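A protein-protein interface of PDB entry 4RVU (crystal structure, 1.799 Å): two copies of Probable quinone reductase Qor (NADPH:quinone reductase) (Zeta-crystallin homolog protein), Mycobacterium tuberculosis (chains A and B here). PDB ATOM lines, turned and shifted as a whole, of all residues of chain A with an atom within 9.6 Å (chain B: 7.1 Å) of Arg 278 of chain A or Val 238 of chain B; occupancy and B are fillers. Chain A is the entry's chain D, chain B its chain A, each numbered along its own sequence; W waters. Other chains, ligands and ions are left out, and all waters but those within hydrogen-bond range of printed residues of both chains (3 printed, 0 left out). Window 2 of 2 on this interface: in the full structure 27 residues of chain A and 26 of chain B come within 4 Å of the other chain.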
ATOM      1  N   SER A  95     -10.662  38.031   8.462  1.00  0.00           N
ATOM      2  CA  SER A  95     -10.891  37.646   7.070  1.00  0.00           C
ATOM      3  C   SER A  95     -10.912  38.854   6.140  1.00  0.00           C
ATOM      4  O   SER A  95     -11.556  38.821   5.091  1.00  0.00           O
ATOM      5  CB  SER A  95     -12.216  36.880   6.942  1.00  0.00           C
ATOM      6  OG  SER A  95     -12.326  35.870   7.931  1.00  0.00           O
ATOM      7  N   SER A 109     -20.255  39.196   7.337  1.00  0.00           N
ATOM      8  CA  SER A 109     -20.597  37.903   7.933  1.00  0.00           C
ATOM      9  C   SER A 109     -19.434  37.300   8.707  1.00  0.00           C
ATOM     10  O   SER A 109     -19.634  36.415   9.521  1.00  0.00           O
ATOM     11  CB  SER A 109     -21.045  36.912   6.856  1.00  0.00           C
ATOM     12  OG  SER A 109     -19.990  36.670   5.942  1.00  0.00           O
ATOM     13  N   LEU A 110     -18.221  37.786   8.450  1.00  0.00           N
ATOM     14  CA  LEU A 110     -17.026  37.309   9.155  1.00  0.00           C
ATOM     15  C   LEU A 110     -16.355  38.431   9.947  1.00  0.00           C
ATOM     16  O   LEU A 110     -15.130  38.451  10.113  1.00  0.00           O
ATOM     17  CB  LEU A 110     -16.039  36.686   8.164  1.00  0.00           C
ATOM     18  CG  LEU A 110     -16.585  35.500   7.370  1.00  0.00           C
ATOM     19  CD1 LEU A 110     -15.553  35.012   6.374  1.00  0.00           C
ATOM     20  CD2 LEU A 110     -16.994  34.367   8.291  1.00  0.00           C
ATOM     21  N   LEU A 131      -9.980  32.466  17.340  1.00  0.00           N
ATOM     22  CA  LEU A 131     -10.853  31.587  16.555  1.00  0.00           C
ATOM     23  C   LEU A 131     -10.113  30.291  16.249  1.00  0.00           C
ATOM     24  O   LEU A 131     -10.695  29.201  16.235  1.00  0.00           O
ATOM     25  CB  LEU A 131     -11.286  32.267  15.247  1.00  0.00           C
ATOM     26  CG  LEU A 131     -12.176  33.505  15.348  1.00  0.00           C
ATOM     27  CD1 LEU A 131     -12.325  34.158  13.970  1.00  0.00           C
ATOM     28  CD2 LEU A 131     -13.544  33.156  15.933  1.00  0.00           C
ATOM     29  N   TYR A 135     -11.294  26.498  17.368  1.00  0.00           N
ATOM     30  CA  TYR A 135     -11.564  25.354  16.498  1.00  0.00           C
ATOM     31  C   TYR A 135     -10.627  24.184  16.820  1.00  0.00           C
ATOM     32  O   TYR A 135     -11.024  23.012  16.725  1.00  0.00           O
ATOM     33  CB  TYR A 135     -11.617  25.752  15.002  1.00  0.00           C
ATOM     34  CG  TYR A 135     -10.312  25.815  14.226  1.00  0.00           C
ATOM     35  CD1 TYR A 135      -9.573  24.664  13.967  1.00  0.00           C
ATOM     36  CD2 TYR A 135      -9.881  27.010  13.655  1.00  0.00           C
ATOM     37  CE1 TYR A 135      -8.405  24.705  13.240  1.00  0.00           C
ATOM     38  CE2 TYR A 135      -8.703  27.062  12.908  1.00  0.00           C
ATOM     39  CZ  TYR A 135      -7.972  25.900  12.712  1.00  0.00           C
ATOM     40  OH  TYR A 135      -6.803  25.920  11.969  1.00  0.00           O
ATOM     41  N   THR A 269      -3.880  15.657  10.948  1.00  0.00           N
ATOM     42  CA  THR A 269      -4.763  16.585  10.252  1.00  0.00           C
ATOM     43  C   THR A 269      -4.064  17.924  10.099  1.00  0.00           C
ATOM     44  O   THR A 269      -3.306  18.341  10.983  1.00  0.00           O
ATOM     45  CB  THR A 269      -6.143  16.733  10.960  1.00  0.00           C
ATOM     46  OG1 THR A 269      -6.983  17.633  10.219  1.00  0.00           O
ATOM     47  CG2 THR A 269      -5.971  17.254  12.375  1.00  0.00           C
ATOM     48  N   PRO A 271      -5.351  21.509   9.561  1.00  0.00           N
ATOM     49  CA  PRO A 271      -6.536  22.360   9.436  1.00  0.00           C
ATOM     50  C   PRO A 271      -6.228  23.800   9.010  1.00  0.00           C
ATOM     51  O   PRO A 271      -5.103  24.288   9.173  1.00  0.00           O
ATOM     52  CB  PRO A 271      -7.124  22.329  10.848  1.00  0.00           C
ATOM     53  CG  PRO A 271      -5.885  22.212  11.751  1.00  0.00           C
ATOM     54  CD  PRO A 271      -4.969  21.278  10.972  1.00  0.00           C
ATOM     55  N   SER A 272      -7.239  24.452   8.442  1.00  0.00           N
ATOM     56  CA  SER A 272      -7.171  25.862   8.052  1.00  0.00           C
ATOM     57  C   SER A 272      -8.391  26.560   8.620  1.00  0.00           C
ATOM     58  O   SER A 272      -9.492  26.019   8.556  1.00  0.00           O
ATOM     59  CB  SER A 272      -7.186  25.977   6.524  1.00  0.00           C
ATOM     60  OG  SER A 272      -7.403  27.311   6.097  1.00  0.00           O
ATOM     61  N   LEU A 273      -8.208  27.768   9.151  1.00  0.00           N
ATOM     62  CA  LEU A 273      -9.320  28.547   9.711  1.00  0.00           C
ATOM     63  C   LEU A 273     -10.481  28.676   8.723  1.00  0.00           C
ATOM     64  O   LEU A 273     -11.641  28.712   9.123  1.00  0.00           O
ATOM     65  CB  LEU A 273      -8.828  29.939  10.159  1.00  0.00           C
ATOM     66  CG  LEU A 273      -9.833  30.908  10.781  1.00  0.00           C
ATOM     67  CD1 LEU A 273     -10.410  30.348  12.058  1.00  0.00           C
ATOM     68  CD2 LEU A 273      -9.167  32.264  11.054  1.00  0.00           C
ATOM     69  N   PHE A 274     -10.163  28.741   7.434  1.00  0.00           N
ATOM     70  CA  PHE A 274     -11.173  28.795   6.379  1.00  0.00           C
ATOM     71  C   PHE A 274     -12.284  27.745   6.530  1.00  0.00           C
ATOM     72  O   PHE A 274     -13.468  28.044   6.331  1.00  0.00           O
ATOM     73  CB  PHE A 274     -10.498  28.669   5.004  1.00  0.00           C
ATOM     74  CG  PHE A 274     -11.466  28.663   3.854  1.00  0.00           C
ATOM     75  CD1 PHE A 274     -11.986  29.850   3.362  1.00  0.00           C
ATOM     76  CD2 PHE A 274     -11.858  27.466   3.268  1.00  0.00           C
ATOM     77  CE1 PHE A 274     -12.886  29.847   2.303  1.00  0.00           C
ATOM     78  CE2 PHE A 274     -12.755  27.451   2.216  1.00  0.00           C
ATOM     79  CZ  PHE A 274     -13.271  28.643   1.731  1.00  0.00           C
ATOM     80  N   HIS A 275     -11.905  26.523   6.898  1.00  0.00           N
ATOM     81  CA  HIS A 275     -12.854  25.423   6.972  1.00  0.00           C
ATOM     82  C   HIS A 275     -13.610  25.388   8.296  1.00  0.00           C
ATOM     83  O   HIS A 275     -14.427  24.491   8.516  1.00  0.00           O
ATOM     84  CB  HIS A 275     -12.145  24.082   6.710  1.00  0.00           C
ATOM     85  CG  HIS A 275     -11.559  23.972   5.335  1.00  0.00           C
ATOM     86  ND1 HIS A 275     -10.216  23.759   5.111  1.00  0.00           N
ATOM     87  CD2 HIS A 275     -12.133  24.066   4.110  1.00  0.00           C
ATOM     88  CE1 HIS A 275      -9.989  23.719   3.808  1.00  0.00           C
ATOM     89  NE2 HIS A 275     -11.135  23.903   3.178  1.00  0.00           N
ATOM     90  N   PHE A 276     -13.338  26.362   9.170  1.00  0.00           N
ATOM     91  CA  PHE A 276     -14.027  26.448  10.458  1.00  0.00           C
ATOM     92  C   PHE A 276     -14.749  27.784  10.633  1.00  0.00           C
ATOM     93  O   PHE A 276     -15.208  28.122  11.734  1.00  0.00           O
ATOM     94  CB  PHE A 276     -13.043  26.185  11.615  1.00  0.00           C
ATOM     95  CG  PHE A 276     -12.362  24.835  11.535  1.00  0.00           C
ATOM     96  CD1 PHE A 276     -12.826  23.756  12.275  1.00  0.00           C
ATOM     97  CD2 PHE A 276     -11.261  24.646  10.703  1.00  0.00           C
ATOM     98  CE1 PHE A 276     -12.197  22.502  12.190  1.00  0.00           C
ATOM     99  CE2 PHE A 276     -10.639  23.406  10.599  1.00  0.00           C
ATOM    100  CZ  PHE A 276     -11.105  22.330  11.356  1.00  0.00           C
ATOM    101  N   THR A 277     -14.835  28.544   9.537  1.00  0.00           N
ATOM    102  CA  THR A 277     -15.590  29.796   9.481  1.00  0.00           C
ATOM    103  C   THR A 277     -16.398  29.800   8.183  1.00  0.00           C
ATOM    104  O   THR A 277     -16.354  30.753   7.399  1.00  0.00           O
ATOM    105  CB  THR A 277     -14.663  31.039   9.537  1.00  0.00           C
ATOM    106  OG1 THR A 277     -13.660  30.938   8.514  1.00  0.00           O
ATOM    107  CG2 THR A 277     -13.966  31.148  10.908  1.00  0.00           C
ATOM    108  N   ARG A 278     -17.127  28.712   7.955  1.00  0.00           N
ATOM    109  CA  ARG A 278     -17.748  28.451   6.663  1.00  0.00           C
ATOM    110  C   ARG A 278     -19.061  29.182   6.477  1.00  0.00           C
ATOM    111  O   ARG A 278     -19.515  29.383   5.350  1.00  0.00           O
ATOM    112  CB  ARG A 278     -17.967  26.949   6.501  1.00  0.00           C
ATOM    113  CG  ARG A 278     -16.682  26.169   6.610  1.00  0.00           C
ATOM    114  CD  ARG A 278     -16.922  24.640   6.742  1.00  0.00           C
ATOM    115  NE  ARG A 278     -17.722  24.031   5.679  1.00  0.00           N
ATOM    116  CZ  ARG A 278     -17.410  24.040   4.385  1.00  0.00           C
ATOM    117  NH1 ARG A 278     -16.319  24.668   3.958  1.00  0.00           N
ATOM    118  NH2 ARG A 278     -18.204  23.429   3.508  1.00  0.00           N
ATOM    119  N   THR A 279     -19.678  29.567   7.584  1.00  0.00           N
ATOM    120  CA  THR A 279     -20.900  30.352   7.535  1.00  0.00           C
ATOM    121  C   THR A 279     -20.744  31.503   8.510  1.00  0.00           C
ATOM    122  O   THR A 279     -19.840  31.481   9.351  1.00  0.00           O
ATOM    123  CB  THR A 279     -22.122  29.530   7.959  1.00  0.00           C
ATOM    124  OG1 THR A 279     -21.925  29.053   9.290  1.00  0.00           O
ATOM    125  CG2 THR A 279     -22.342  28.335   7.024  1.00  0.00           C
ATOM    126  N   GLY A 280     -21.626  32.496   8.407  1.00  0.00           N
ATOM    127  CA  GLY A 280     -21.668  33.563   9.395  1.00  0.00           C
ATOM    128  C   GLY A 280     -22.054  32.993  10.749  1.00  0.00           C
ATOM    129  O   GLY A 280     -21.563  33.442  11.786  1.00  0.00           O
ATOM    130  N   GLU A 281     -22.930  31.989  10.731  1.00  0.00           N
ATOM    131  CA  GLU A 281     -23.398  31.327  11.949  1.00  0.00           C
ATOM    132  C   GLU A 281     -22.249  30.656  12.692  1.00  0.00           C
ATOM    133  O   GLU A 281     -22.136  30.740  13.917  1.00  0.00           O
ATOM    134  CB  GLU A 281     -24.457  30.269  11.604  1.00  0.00           C
ATOM    135  CG  GLU A 281     -25.784  30.824  11.061  1.00  0.00           C
ATOM    136  CD  GLU A 281     -25.679  31.449   9.661  1.00  0.00           C
ATOM    137  OE1 GLU A 281     -24.774  31.064   8.882  1.00  0.00           O
ATOM    138  OE2 GLU A 281     -26.512  32.331   9.341  1.00  0.00           O
ATOM    139  N   GLU A 282     -21.394  29.986  11.933  1.00  0.00           N
ATOM    140  CA  GLU A 282     -20.240  29.311  12.498  1.00  0.00           C
ATOM    141  C   GLU A 282     -19.260  30.333  13.079  1.00  0.00           C
ATOM    142  O   GLU A 282     -18.774  30.177  14.209  1.00  0.00           O
ATOM    143  CB  GLU A 282     -19.550  28.452  11.428  1.00  0.00           C
ATOM    144  CG  GLU A 282     -18.483  27.551  12.027  1.00  0.00           C
ATOM    145  CD  GLU A 282     -17.842  26.541  11.079  1.00  0.00           C
ATOM    146  OE1 GLU A 282     -17.849  26.764   9.857  1.00  0.00           O
ATOM    147  OE2 GLU A 282     -17.320  25.516  11.577  1.00  0.00           O
ATOM    148  N   PHE A 283     -18.982  31.374  12.305  1.00  0.00           N
ATOM    149  CA  PHE A 283     -18.089  32.440  12.753  1.00  0.00           C
ATOM    150  C   PHE A 283     -18.608  33.049  14.050  1.00  0.00           C
ATOM    151  O   PHE A 283     -17.852  33.271  14.996  1.00  0.00           O
ATOM    152  CB  PHE A 283     -17.963  33.528  11.689  1.00  0.00           C
ATOM    153  CG  PHE A 283     -17.274  34.768  12.187  1.00  0.00           C
ATOM    154  CD1 PHE A 283     -15.889  34.847  12.197  1.00  0.00           C
ATOM    155  CD2 PHE A 283     -18.010  35.855  12.657  1.00  0.00           C
ATOM    156  CE1 PHE A 283     -15.236  35.987  12.684  1.00  0.00           C
ATOM    157  CE2 PHE A 283     -17.373  36.995  13.152  1.00  0.00           C
ATOM    158  CZ  PHE A 283     -15.979  37.069  13.162  1.00  0.00           C
ATOM    159  N   SER A 284     -19.903  33.329  14.080  1.00  0.00           N
ATOM    160  CA  SER A 284     -20.496  34.033  15.210  1.00  0.00           C
ATOM    161  C   SER A 284     -20.438  33.201  16.483  1.00  0.00           C
ATOM    162  O   SER A 284     -20.222  33.731  17.572  1.00  0.00           O
ATOM    163  CB  SER A 284     -21.932  34.445  14.890  1.00  0.00           C
ATOM    164  OG  SER A 284     -21.914  35.556  14.020  1.00  0.00           O
ATOM    165  N   TRP A 285     -20.631  31.899  16.327  1.00  0.00           N
ATOM    166  CA  TRP A 285     -20.556  30.962  17.439  1.00  0.00           C
ATOM    167  C   TRP A 285     -19.158  30.965  18.038  1.00  0.00           C
ATOM    168  O   TRP A 285     -18.997  31.077  19.252  1.00  0.00           O
ATOM    169  CB  TRP A 285     -20.934  29.551  16.970  1.00  0.00           C
ATOM    170  CG  TRP A 285     -20.575  28.461  17.954  1.00  0.00           C
ATOM    171  CD1 TRP A 285     -20.954  28.378  19.262  1.00  0.00           C
ATOM    172  CD2 TRP A 285     -19.781  27.292  17.692  1.00  0.00           C
ATOM    173  NE1 TRP A 285     -20.433  27.239  19.831  1.00  0.00           N
ATOM    174  CE2 TRP A 285     -19.714  26.556  18.889  1.00  0.00           C
ATOM    175  CE3 TRP A 285     -19.127  26.802  16.561  1.00  0.00           C
ATOM    176  CZ2 TRP A 285     -19.008  25.350  18.986  1.00  0.00           C
ATOM    177  CZ3 TRP A 285     -18.426  25.605  16.661  1.00  0.00           C
ATOM    178  CH2 TRP A 285     -18.377  24.891  17.859  1.00  0.00           C
ATOM    179  N   ARG A 286     -18.143  30.831  17.186  1.00  0.00           N
ATOM    180  CA  ARG A 286     -16.772  30.748  17.672  1.00  0.00           C
ATOM    181  C   ARG A 286     -16.354  32.075  18.285  1.00  0.00           C
ATOM    182  O   ARG A 286     -15.742  32.113  19.347  1.00  0.00           O
ATOM    183  CB  ARG A 286     -15.817  30.344  16.543  1.00  0.00           C
ATOM    184  CG  ARG A 286     -15.935  28.888  16.102  1.00  0.00           C
ATOM    185  CD  ARG A 286     -14.880  28.546  15.024  1.00  0.00           C
ATOM    186  NE  ARG A 286     -14.809  27.134  14.593  1.00  0.00           N
ATOM    187  CZ  ARG A 286     -15.835  26.360  14.258  1.00  0.00           C
ATOM    188  NH1 ARG A 286     -17.062  26.822  14.345  1.00  0.00           N
ATOM    189  NH2 ARG A 286     -15.640  25.084  13.913  1.00  0.00           N
ATOM    190  N   ARG B 209     -18.504  13.333  -6.085  1.00  0.00           N
ATOM    191  CA  ARG B 209     -19.189  14.595  -5.814  1.00  0.00           C
ATOM    192  C   ARG B 209     -20.581  14.604  -6.452  1.00  0.00           C
ATOM    193  O   ARG B 209     -21.553  15.016  -5.817  1.00  0.00           O
ATOM    194  CB  ARG B 209     -18.373  15.798  -6.314  1.00  0.00           C
ATOM    195  CG  ARG B 209     -16.973  15.909  -5.716  1.00  0.00           C
ATOM    196  CD  ARG B 209     -16.801  17.033  -4.705  1.00  0.00           C
ATOM    197  NE  ARG B 209     -15.511  16.915  -4.021  1.00  0.00           N
ATOM    198  CZ  ARG B 209     -15.344  17.013  -2.706  1.00  0.00           C
ATOM    199  NH1 ARG B 209     -16.380  17.260  -1.917  1.00  0.00           N
ATOM    200  NH2 ARG B 209     -14.136  16.867  -2.183  1.00  0.00           N
ATOM    201  N   THR B 215     -20.827  17.478  -2.102  1.00  0.00           N
ATOM    202  CA  THR B 215     -20.355  17.432  -0.711  1.00  0.00           C
ATOM    203  C   THR B 215     -19.115  16.568  -0.526  1.00  0.00           C
ATOM    204  O   THR B 215     -18.177  16.946   0.185  1.00  0.00           O
ATOM    205  CB  THR B 215     -21.445  16.926   0.254  1.00  0.00           C
ATOM    206  OG1 THR B 215     -22.632  17.710   0.098  1.00  0.00           O
ATOM    207  CG2 THR B 215     -20.970  17.019   1.706  1.00  0.00           C
ATOM    208  N   GLY B 216     -19.097  15.413  -1.180  1.00  0.00           N
ATOM    209  CA  GLY B 216     -18.067  14.429  -0.915  1.00  0.00           C
ATOM    210  C   GLY B 216     -18.541  13.509   0.195  1.00  0.00           C
ATOM    211  O   GLY B 216     -19.606  13.735   0.785  1.00  0.00           O
ATOM    212  N   VAL B 217     -17.751  12.479   0.487  1.00  0.00           N
ATOM    213  CA  VAL B 217     -18.110  11.494   1.508  1.00  0.00           C
ATOM    214  C   VAL B 217     -17.582  11.854   2.912  1.00  0.00           C
ATOM    215  O   VAL B 217     -16.546  12.501   3.043  1.00  0.00           O
ATOM    216  CB  VAL B 217     -17.644  10.073   1.096  1.00  0.00           C
ATOM    217  CG1 VAL B 217     -18.456   9.556  -0.110  1.00  0.00           C
ATOM    218  CG2 VAL B 217     -16.147  10.056   0.798  1.00  0.00           C
ATOM    219  N   GLN B 218     -18.297  11.441   3.956  1.00  0.00           N
ATOM    220  CA  GLN B 218     -17.866  11.732   5.327  1.00  0.00           C
ATOM    221  C   GLN B 218     -16.594  10.971   5.707  1.00  0.00           C
ATOM    222  O   GLN B 218     -15.837  11.399   6.594  1.00  0.00           O
ATOM    223  CB  GLN B 218     -18.983  11.438   6.335  1.00  0.00           C
ATOM    224  CG  GLN B 218     -19.976  12.582   6.510  1.00  0.00           C
ATOM    225  CD  GLN B 218     -20.841  12.799   5.287  1.00  0.00           C
ATOM    226  OE1 GLN B 218     -21.426  11.852   4.749  1.00  0.00           O
ATOM    227  NE2 GLN B 218     -20.920  14.050   4.830  1.00  0.00           N
ATOM    228  N   LEU B 236     -13.249  13.578  -0.374  1.00  0.00           N
ATOM    229  CA  LEU B 236     -13.745  13.804   0.988  1.00  0.00           C
ATOM    230  C   LEU B 236     -14.564  15.072   1.222  1.00  0.00           C
ATOM    231  O   LEU B 236     -14.300  16.127   0.642  1.00  0.00           O
ATOM    232  CB  LEU B 236     -12.578  13.820   1.968  1.00  0.00           C
ATOM    233  CG  LEU B 236     -12.009  12.448   2.293  1.00  0.00           C
ATOM    234  CD1 LEU B 236     -10.608  12.599   2.851  1.00  0.00           C
ATOM    235  CD2 LEU B 236     -12.910  11.751   3.303  1.00  0.00           C
ATOM    236  N   ALA B 237     -15.543  14.961   2.110  1.00  0.00           N
ATOM    237  CA  ALA B 237     -16.272  16.128   2.579  1.00  0.00           C
ATOM    238  C   ALA B 237     -15.336  16.926   3.472  1.00  0.00           C
ATOM    239  O   ALA B 237     -14.316  16.401   3.937  1.00  0.00           O
ATOM    240  CB  ALA B 237     -17.500  15.712   3.346  1.00  0.00           C
ATOM    241  N   VAL B 238     -15.673  18.191   3.707  1.00  0.00           N
ATOM    242  CA  VAL B 238     -14.869  19.039   4.592  1.00  0.00           C
ATOM    243  C   VAL B 238     -14.743  18.383   5.967  1.00  0.00           C
ATOM    244  O   VAL B 238     -15.746  17.944   6.547  1.00  0.00           O
ATOM    245  CB  VAL B 238     -15.480  20.461   4.728  1.00  0.00           C
ATOM    246  CG1 VAL B 238     -14.737  21.277   5.803  1.00  0.00           C
ATOM    247  CG2 VAL B 238     -15.442  21.176   3.390  1.00  0.00           C
ATOM    248  N   ARG B 239     -13.505  18.298   6.460  1.00  0.00           N
ATOM    249  CA  ARG B 239     -13.193  17.718   7.763  1.00  0.00           C
ATOM    250  C   ARG B 239     -13.487  16.217   7.828  1.00  0.00           C
ATOM    251  O   ARG B 239     -13.643  15.650   8.914  1.00  0.00           O
ATOM    252  CB  ARG B 239     -13.908  18.470   8.890  1.00  0.00           C
ATOM    253  CG  ARG B 239     -13.344  19.898   9.113  1.00  0.00           C
ATOM    254  CD  ARG B 239     -14.248  20.704  10.041  1.00  0.00           C
ATOM    255  NE  ARG B 239     -14.411  20.048  11.337  1.00  0.00           N
ATOM    256  CZ  ARG B 239     -15.340  20.372  12.235  1.00  0.00           C
ATOM    257  NH1 ARG B 239     -16.196  21.358  11.993  1.00  0.00           N
ATOM    258  NH2 ARG B 239     -15.407  19.716  13.383  1.00  0.00           N
ATOM    259  N   GLY B 240     -13.528  15.584   6.659  1.00  0.00           N
ATOM    260  CA  GLY B 240     -13.810  14.160   6.567  1.00  0.00           C
ATOM    261  C   GLY B 240     -12.603  13.333   6.969  1.00  0.00           C
ATOM    262  O   GLY B 240     -11.519  13.866   7.179  1.00  0.00           O
ATOM    263  N   THR B 241     -12.780  12.019   7.076  1.00  0.00           N
ATOM    264  CA  THR B 241     -11.692  11.154   7.545  1.00  0.00           C
ATOM    265  C   THR B 241     -11.273  10.169   6.467  1.00  0.00           C
ATOM    266  O   THR B 241     -12.099   9.409   5.967  1.00  0.00           O
ATOM    267  CB  THR B 241     -12.112  10.356   8.794  1.00  0.00           C
ATOM    268  OG1 THR B 241     -12.308  11.248   9.900  1.00  0.00           O
ATOM    269  CG2 THR B 241     -11.044   9.321   9.160  1.00  0.00           C
ATOM    270  N   ALA B 263      -7.491  19.573   0.749  1.00  0.00           N
ATOM    271  CA  ALA B 263      -8.579  18.623   0.544  1.00  0.00           C
ATOM    272  C   ALA B 263      -9.799  18.940   1.401  1.00  0.00           C
ATOM    273  O   ALA B 263     -10.860  18.357   1.203  1.00  0.00           O
ATOM    274  CB  ALA B 263      -8.095  17.202   0.805  1.00  0.00           C
ATOM    275  N   GLY B 264      -9.649  19.861   2.354  1.00  0.00           N
ATOM    276  CA  GLY B 264     -10.755  20.232   3.229  1.00  0.00           C
ATOM    277  C   GLY B 264     -10.498  20.130   4.731  1.00  0.00           C
ATOM    278  O   GLY B 264     -11.436  19.865   5.499  1.00  0.00           O
ATOM    279  N   SER B 265      -9.262  20.392   5.161  1.00  0.00           N
ATOM    280  CA  SER B 265      -8.870  20.211   6.572  1.00  0.00           C
ATOM    281  C   SER B 265      -9.306  18.833   7.052  1.00  0.00           C
ATOM    282  O   SER B 265     -10.004  18.687   8.066  1.00  0.00           O
ATOM    283  CB  SER B 265      -9.460  21.303   7.468  1.00  0.00           C
ATOM    284  OG  SER B 265      -8.934  22.578   7.137  1.00  0.00           O
ATOM    285  N   VAL B 266      -8.891  17.819   6.309  1.00  0.00           N
ATOM    286  CA  VAL B 266      -9.356  16.469   6.571  1.00  0.00           C
ATOM    287  C   VAL B 266      -8.410  15.771   7.529  1.00  0.00           C
ATOM    288  O   VAL B 266      -7.338  16.290   7.850  1.00  0.00           O
ATOM    289  CB  VAL B 266      -9.463  15.665   5.276  1.00  0.00           C
ATOM    290  CG1 VAL B 266     -10.311  16.429   4.266  1.00  0.00           C
ATOM    291  CG2 VAL B 266      -8.082  15.383   4.711  1.00  0.00           C
HETATM  292  O   HOH W   1      -9.425  19.157  10.761  1.00  0.00           O
HETATM  293  O   HOH W   2     -17.640  22.621  14.367  1.00  0.00           O
HETATM  294  O   HOH W   3     -16.264  23.453  10.106  1.00  0.00           O
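No position is printed for both chains.
Of the 10 pairs that touch across the chains among the printed residues, none has its exchanged pair printed and touching as well.
Water W3 lies within hydrogen-bond range of O of His 275 of chain A (2.6 Å), OE2 of Glu 282 of chain A (2.7 Å) and NH1 of Arg 239 of chain B (2.8 Å).
Water W1 lies within hydrogen-bond range of O of Ser 265 of chain B (2.8 Å) and OG1 of Thr 269 of chain A (2.9 Å).
Water W2 bridges NH1 of Arg 239 of chain B and NH2 of Arg 286 of chain A.
Hydrophobic or aromatic side chains of chain B within 4 Å of the printed part of chain A: Val 238.
Hydrophobic or aromatic side chains of chain A that line the printed part of chain B: His 275 and Phe 276.
OG of Ser 272 of chain A sits close to N of Phe 274 of chain A, 3.4 Å away.
The backbone NH (N) of Arg 278 of chain A lies within hydrogen-bond range of the side-chain carboxylate (OE1) of Glu 282 of chain A (2.8 Å).
O of Phe 276 of chain A sits at hydrogen-bond distance from NE of Arg 286 of chain A (3.1 Å).
The backbone carbonyl oxygen (O) of Gly 264 of chain B sits at hydrogen-bond distance from the backbone NH (N) of Arg 239 of chain B, at 2.8 Å.
Ser 265 of chain B touches Thr 269 of chain A (O to OG1, 3.9 Å).
OG of Ser 265 of chain B touches CA of Pro 271 of chain A, 3.3 Å away.
His 275 of chain A touches Val 238 of chain B (CB to CG1, 3.9 Å).
CA of Gly 264 of chain B touches CE1 of His 275 of chain A (3.6 Å).
Phe 276 of chain A touches Arg 239 of chain B.
OG of Ser 265 of chain B touches CE2 of Phe 276 of chain A (3.9 Å).
Val 238 of chain B touches Arg 278 of chain A.
The side-chain hydroxyl of Thr 269 of chain A lies within hydrogen-bond range of the backbone carbonyl oxygen of Val 266 of chain B (2.7 Å).
A ring nitrogen (ND1) of His 275 of chain A is in hydrogen-bond range of the side-chain hydroxyl of Ser 265 of chain B.
The backbone NH of Ser 272 of chain A is in hydrogen-bond range of the side-chain hydroxyl of Ser 265 of chain B (2.8 Å).
Of chain B, only Val 238 (3.6 Å) comes within 4 Å of Arg 278 of chain A.
No residue of chain A comes within 4 Å of Ala 237 of chain B.
Val 238 of chain B touches just these residues of chain A: His 275 (3.9 Å) and Arg 278 (3.6 Å).
Printed residues of chain A within 4 Å of Arg 239 of chain B: Phe 276 (3.4 Å).
Printed residues of chain A within 4 Å of Ser 265 of chain B: Thr 269 (3.9 Å), Pro 271 (3.3 Å), Ser 272 (2.8 Å), His 275 (2.7 Å) and Phe 276 (3.9 Å).
The nearest printed residue of chain A that does not touch Val 266 of chain B is Pro 271 of chain A (5.8 Å).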
